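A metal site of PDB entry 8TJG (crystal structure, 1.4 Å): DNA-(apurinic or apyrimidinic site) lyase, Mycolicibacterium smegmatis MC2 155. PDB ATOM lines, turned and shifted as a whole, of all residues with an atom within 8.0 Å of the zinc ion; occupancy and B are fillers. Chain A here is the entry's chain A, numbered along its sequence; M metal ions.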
ATOM      1  N   PHE A 167       7.906 -20.029  -8.961  1.00  0.00           N
ATOM      2  CA  PHE A 167       8.181 -20.883 -10.109  1.00  0.00           C
ATOM      3  C   PHE A 167       6.920 -21.234 -10.879  1.00  0.00           C
ATOM      4  O   PHE A 167       6.873 -21.094 -12.120  1.00  0.00           O
ATOM      5  CB  PHE A 167       8.911 -22.166  -9.702  1.00  0.00           C
ATOM      6  CG  PHE A 167       9.011 -23.154 -10.847  1.00  0.00           C
ATOM      7  CD1 PHE A 167       9.977 -23.002 -11.863  1.00  0.00           C
ATOM      8  CD2 PHE A 167       8.094 -24.188 -10.963  1.00  0.00           C
ATOM      9  CE1 PHE A 167      10.048 -23.896 -12.939  1.00  0.00           C
ATOM     10  CE2 PHE A 167       8.134 -25.073 -12.044  1.00  0.00           C
ATOM     11  CZ  PHE A 167       9.121 -24.949 -13.033  1.00  0.00           C
ATOM     12  N   TRP A 216       9.798 -28.207  -7.162  1.00  0.00           N
ATOM     13  CA  TRP A 216      10.180 -27.692  -8.489  1.00  0.00           C
ATOM     14  C   TRP A 216      11.554 -27.050  -8.478  1.00  0.00           C
ATOM     15  O   TRP A 216      12.364 -27.289  -9.386  1.00  0.00           O
ATOM     16  CB  TRP A 216       9.179 -26.651  -8.974  1.00  0.00           C
ATOM     17  CG  TRP A 216       7.800 -27.227  -9.210  1.00  0.00           C
ATOM     18  CD1 TRP A 216       6.711 -27.044  -8.402  1.00  0.00           C
ATOM     19  CD2 TRP A 216       7.373 -28.070 -10.288  1.00  0.00           C
ATOM     20  NE1 TRP A 216       5.636 -27.751  -8.914  1.00  0.00           N
ATOM     21  CE2 TRP A 216       6.010 -28.384 -10.062  1.00  0.00           C
ATOM     22  CE3 TRP A 216       8.010 -28.621 -11.405  1.00  0.00           C
ATOM     23  CZ2 TRP A 216       5.269 -29.198 -10.930  1.00  0.00           C
ATOM     24  CZ3 TRP A 216       7.270 -29.435 -12.273  1.00  0.00           C
ATOM     25  CH2 TRP A 216       5.917 -29.715 -12.026  1.00  0.00           C
ATOM     26  N   VAL A 217      11.818 -26.145  -7.527  1.00  0.00           N
ATOM     27  CA  VAL A 217      13.063 -25.384  -7.538  1.00  0.00           C
ATOM     28  C   VAL A 217      13.752 -25.314  -6.185  1.00  0.00           C
ATOM     29  O   VAL A 217      14.972 -25.264  -6.130  1.00  0.00           O
ATOM     30  CB  VAL A 217      12.864 -23.952  -8.102  1.00  0.00           C
ATOM     31  CG1 VAL A 217      12.412 -24.018  -9.573  1.00  0.00           C
ATOM     32  CG2 VAL A 217      11.896 -23.115  -7.227  1.00  0.00           C
ATOM     33  N   PRO A 224      18.362 -29.924 -13.076  1.00  0.00           N
ATOM     34  CA  PRO A 224      17.519 -29.509 -14.196  1.00  0.00           C
ATOM     35  C   PRO A 224      16.122 -29.139 -13.748  1.00  0.00           C
ATOM     36  O   PRO A 224      15.492 -29.844 -12.947  1.00  0.00           O
ATOM     37  CB  PRO A 224      17.495 -30.740 -15.119  1.00  0.00           C
ATOM     38  CG  PRO A 224      18.496 -31.690 -14.595  1.00  0.00           C
ATOM     39  CD  PRO A 224      18.773 -31.346 -13.166  1.00  0.00           C
ATOM     40  N   CYS A 225      15.608 -28.054 -14.320  1.00  0.00           N
ATOM     41  CA  CYS A 225      14.197 -27.771 -14.193  1.00  0.00           C
ATOM     42  C   CYS A 225      13.416 -28.978 -14.723  1.00  0.00           C
ATOM     43  O   CYS A 225      13.745 -29.524 -15.787  1.00  0.00           O
ATOM     44  CB  CYS A 225      13.890 -26.535 -15.018  1.00  0.00           C
ATOM     45  SG  CYS A 225      12.109 -26.132 -15.100  1.00  0.00           S
ATOM     46  N   ARG A 226      12.395 -29.390 -13.974  1.00  0.00           N
ATOM     47  CA  ARG A 226      11.632 -30.579 -14.312  1.00  0.00           C
ATOM     48  C   ARG A 226      10.795 -30.426 -15.561  1.00  0.00           C
ATOM     49  O   ARG A 226      10.363 -31.438 -16.119  1.00  0.00           O
ATOM     50  CB  ARG A 226      10.725 -30.930 -13.152  1.00  0.00           C
ATOM     51  CG  ARG A 226      11.492 -31.148 -11.863  1.00  0.00           C
ATOM     52  CD  ARG A 226      10.605 -31.769 -10.862  1.00  0.00           C
ATOM     53  NE  ARG A 226      11.215 -31.768  -9.533  1.00  0.00           N
ATOM     54  CZ  ARG A 226      12.064 -32.685  -9.089  1.00  0.00           C
ATOM     55  NH1 ARG A 226      12.466 -33.699  -9.861  1.00  0.00           N
ATOM     56  NH2 ARG A 226      12.509 -32.594  -7.851  1.00  0.00           N
ATOM     57  N   ARG A 227      10.556 -29.199 -15.987  1.00  0.00           N
ATOM     58  CA  ARG A 227       9.839 -28.928 -17.221  1.00  0.00           C
ATOM     59  C   ARG A 227      10.826 -28.683 -18.356  1.00  0.00           C
ATOM     60  O   ARG A 227      10.982 -29.543 -19.239  1.00  0.00           O
ATOM     61  CB  ARG A 227       8.899 -27.722 -17.018  1.00  0.00           C
ATOM     62  CG  ARG A 227       7.713 -28.032 -16.068  1.00  0.00           C
ATOM     63  CD  ARG A 227       6.815 -29.160 -16.607  1.00  0.00           C
ATOM     64  NE  ARG A 227       5.477 -29.120 -16.032  1.00  0.00           N
ATOM     65  CZ  ARG A 227       4.874 -30.167 -15.478  1.00  0.00           C
ATOM     66  NH1 ARG A 227       5.456 -31.350 -15.411  1.00  0.00           N
ATOM     67  NH2 ARG A 227       3.655 -30.019 -14.952  1.00  0.00           N
ATOM     68  N   CYS A 228      11.533 -27.532 -18.355  1.00  0.00           N
ATOM     69  CA  CYS A 228      12.300 -27.139 -19.538  1.00  0.00           C
ATOM     70  C   CYS A 228      13.695 -27.749 -19.610  1.00  0.00           C
ATOM     71  O   CYS A 228      14.318 -27.730 -20.680  1.00  0.00           O
ATOM     72  CB  CYS A 228      12.410 -25.604 -19.628  1.00  0.00           C
ATOM     73  SG  CYS A 228      13.511 -24.910 -18.401  1.00  0.00           S
ATOM     74  N   GLY A 229      14.206 -28.303 -18.504  1.00  0.00           N
ATOM     75  CA  GLY A 229      15.516 -28.911 -18.498  1.00  0.00           C
ATOM     76  C   GLY A 229      16.665 -28.003 -18.113  1.00  0.00           C
ATOM     77  O   GLY A 229      17.768 -28.507 -17.868  1.00  0.00           O
ATOM     78  N   THR A 230      16.446 -26.689 -18.034  1.00  0.00           N
ATOM     79  CA  THR A 230      17.513 -25.726 -17.762  1.00  0.00           C
ATOM     80  C   THR A 230      17.968 -25.885 -16.305  1.00  0.00           C
ATOM     81  O   THR A 230      17.160 -26.143 -15.412  1.00  0.00           O
ATOM     82  CB  THR A 230      16.908 -24.332 -17.934  1.00  0.00           C
ATOM     83  OG1 THR A 230      16.509 -24.148 -19.316  1.00  0.00           O
ATOM     84  CG2 THR A 230      17.885 -23.239 -17.573  1.00  0.00           C
ATOM     85  N   LEU A 231      19.250 -25.687 -16.052  1.00  0.00           N
ATOM     86  CA  LEU A 231      19.713 -25.803 -14.666  1.00  0.00           C
ATOM     87  C   LEU A 231      19.159 -24.670 -13.786  1.00  0.00           C
ATOM     88  O   LEU A 231      19.177 -23.490 -14.170  1.00  0.00           O
ATOM     89  CB  LEU A 231      21.240 -25.806 -14.623  1.00  0.00           C
ATOM     90  CG  LEU A 231      21.917 -26.953 -15.364  1.00  0.00           C
ATOM     91  CD1 LEU A 231      23.429 -26.877 -15.105  1.00  0.00           C
ATOM     92  CD2 LEU A 231      21.343 -28.317 -14.950  1.00  0.00           C
ATOM     93  N   ILE A 232      18.711 -25.041 -12.584  1.00  0.00           N
ATOM     94  CA  ILE A 232      18.177 -24.083 -11.611  1.00  0.00           C
ATOM     95  C   ILE A 232      19.283 -23.221 -11.019  1.00  0.00           C
ATOM     96  O   ILE A 232      20.385 -23.698 -10.709  1.00  0.00           O
ATOM     97  CB  ILE A 232      17.398 -24.867 -10.524  1.00  0.00           C
ATOM     98  CG1 ILE A 232      16.234 -25.663 -11.166  1.00  0.00           C
ATOM     99  CG2 ILE A 232      16.950 -23.975  -9.347  1.00  0.00           C
ATOM    100  CD1 ILE A 232      15.364 -24.881 -12.074  1.00  0.00           C
ATOM    101  N   TRP A 244      15.477 -20.443  -8.704  1.00  0.00           N
ATOM    102  CA  TRP A 244      14.580 -20.176  -9.824  1.00  0.00           C
ATOM    103  C   TRP A 244      15.120 -20.804 -11.093  1.00  0.00           C
ATOM    104  O   TRP A 244      16.317 -21.073 -11.216  1.00  0.00           O
ATOM    105  CB  TRP A 244      14.350 -18.662 -10.022  1.00  0.00           C
ATOM    106  CG  TRP A 244      15.516 -17.938 -10.603  1.00  0.00           C
ATOM    107  CD1 TRP A 244      15.733 -17.620 -11.923  1.00  0.00           C
ATOM    108  CD2 TRP A 244      16.637 -17.404  -9.873  1.00  0.00           C
ATOM    109  NE1 TRP A 244      16.924 -16.945 -12.060  1.00  0.00           N
ATOM    110  CE2 TRP A 244      17.500 -16.793 -10.823  1.00  0.00           C
ATOM    111  CE3 TRP A 244      16.993 -17.382  -8.523  1.00  0.00           C
ATOM    112  CZ2 TRP A 244      18.691 -16.183 -10.444  1.00  0.00           C
ATOM    113  CZ3 TRP A 244      18.175 -16.784  -8.158  1.00  0.00           C
ATOM    114  CH2 TRP A 244      19.018 -16.185  -9.114  1.00  0.00           C
ATOM    115  N   CYS A 245      14.197 -21.097 -12.015  1.00  0.00           N
ATOM    116  CA  CYS A 245      14.574 -21.520 -13.342  1.00  0.00           C
ATOM    117  C   CYS A 245      14.683 -20.287 -14.214  1.00  0.00           C
ATOM    118  O   CYS A 245      13.702 -19.542 -14.348  1.00  0.00           O
ATOM    119  CB  CYS A 245      13.529 -22.436 -13.941  1.00  0.00           C
ATOM    120  SG  CYS A 245      13.889 -22.822 -15.677  1.00  0.00           S
ATOM    121  N   PRO A 246      15.841 -20.021 -14.822  1.00  0.00           N
ATOM    122  CA  PRO A 246      15.993 -18.788 -15.605  1.00  0.00           C
ATOM    123  C   PRO A 246      15.289 -18.807 -16.949  1.00  0.00           C
ATOM    124  O   PRO A 246      15.227 -17.757 -17.593  1.00  0.00           O
ATOM    125  CB  PRO A 246      17.513 -18.657 -15.742  1.00  0.00           C
ATOM    126  CG  PRO A 246      18.022 -20.044 -15.633  1.00  0.00           C
ATOM    127  CD  PRO A 246      17.096 -20.775 -14.703  1.00  0.00           C
ATOM    128  N   VAL A 247      14.740 -19.937 -17.380  1.00  0.00           N
ATOM    129  CA  VAL A 247      13.893 -19.983 -18.571  1.00  0.00           C
ATOM    130  C   VAL A 247      12.413 -19.869 -18.217  1.00  0.00           C
ATOM    131  O   VAL A 247      11.657 -19.119 -18.837  1.00  0.00           O
ATOM    132  CB  VAL A 247      14.206 -21.250 -19.408  1.00  0.00           C
ATOM    133  CG1 VAL A 247      13.098 -21.558 -20.451  1.00  0.00           C
ATOM    134  CG2 VAL A 247      15.593 -21.139 -20.067  1.00  0.00           C
ATOM    135  N   CYS A 248      11.954 -20.633 -17.225  1.00  0.00           N
ATOM    136  CA  CYS A 248      10.542 -20.585 -16.857  1.00  0.00           C
ATOM    137  C   CYS A 248      10.191 -19.329 -16.088  1.00  0.00           C
ATOM    138  O   CYS A 248       9.014 -18.950 -16.083  1.00  0.00           O
ATOM    139  CB  CYS A 248      10.148 -21.812 -16.048  1.00  0.00           C
ATOM    140  SG  CYS A 248      10.220 -23.397 -16.918  1.00  0.00           S
ATOM    141  N   GLN A 249      11.167 -18.692 -15.443  1.00  0.00           N
ATOM    142  CA  GLN A 249      10.953 -17.485 -14.644  1.00  0.00           C
ATOM    143  C   GLN A 249      11.793 -16.366 -15.257  1.00  0.00           C
ATOM    144  O   GLN A 249      12.999 -16.272 -15.016  1.00  0.00           O
ATOM    145  CB  GLN A 249      11.334 -17.731 -13.184  1.00  0.00           C
ATOM    146  CG  GLN A 249      10.430 -18.753 -12.513  1.00  0.00           C
ATOM    147  CD  GLN A 249      10.968 -19.186 -11.163  1.00  0.00           C
ATOM    148  OE1 GLN A 249      11.602 -20.252 -11.040  1.00  0.00           O
ATOM    149  NE2 GLN A 249      10.679 -18.393 -10.144  1.00  0.00           N
HETATM  150 ZN    ZN M   1      12.320 -24.277 -16.500  1.00  0.00          ZN
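The nearest printed residue that does not touch the zinc ion is Phe 167 (4.2 Å).
The zinc ion is bound by the side-chain sulfur (SG) of Cys 245, the side-chain sulfur (SG) of Cys 248, the side-chain sulfur (SG) of Cys 228 and the side-chain sulfur (SG) of Cys 225.
The side-chain sulfur of Cys 245 sits close to the backbone NH of Val 247, 3.5 Å away. The backbone NH of Cys 245 is in hydrogen-bond range of the side-chain amide oxygen of Gln 249 (2.9 Å). The side-chain sulfur of Cys 228 sits close to the side-chain hydroxyl of Thr 230, at 3.2 Å. The backbone NH (N) of Cys 225 lies within hydrogen-bond range of the backbone carbonyl oxygen (O) of Thr 230. The side-chain sulfur (SG) of Cys 225 lies close to the backbone NH (N) of Arg 227 (3.6 Å).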
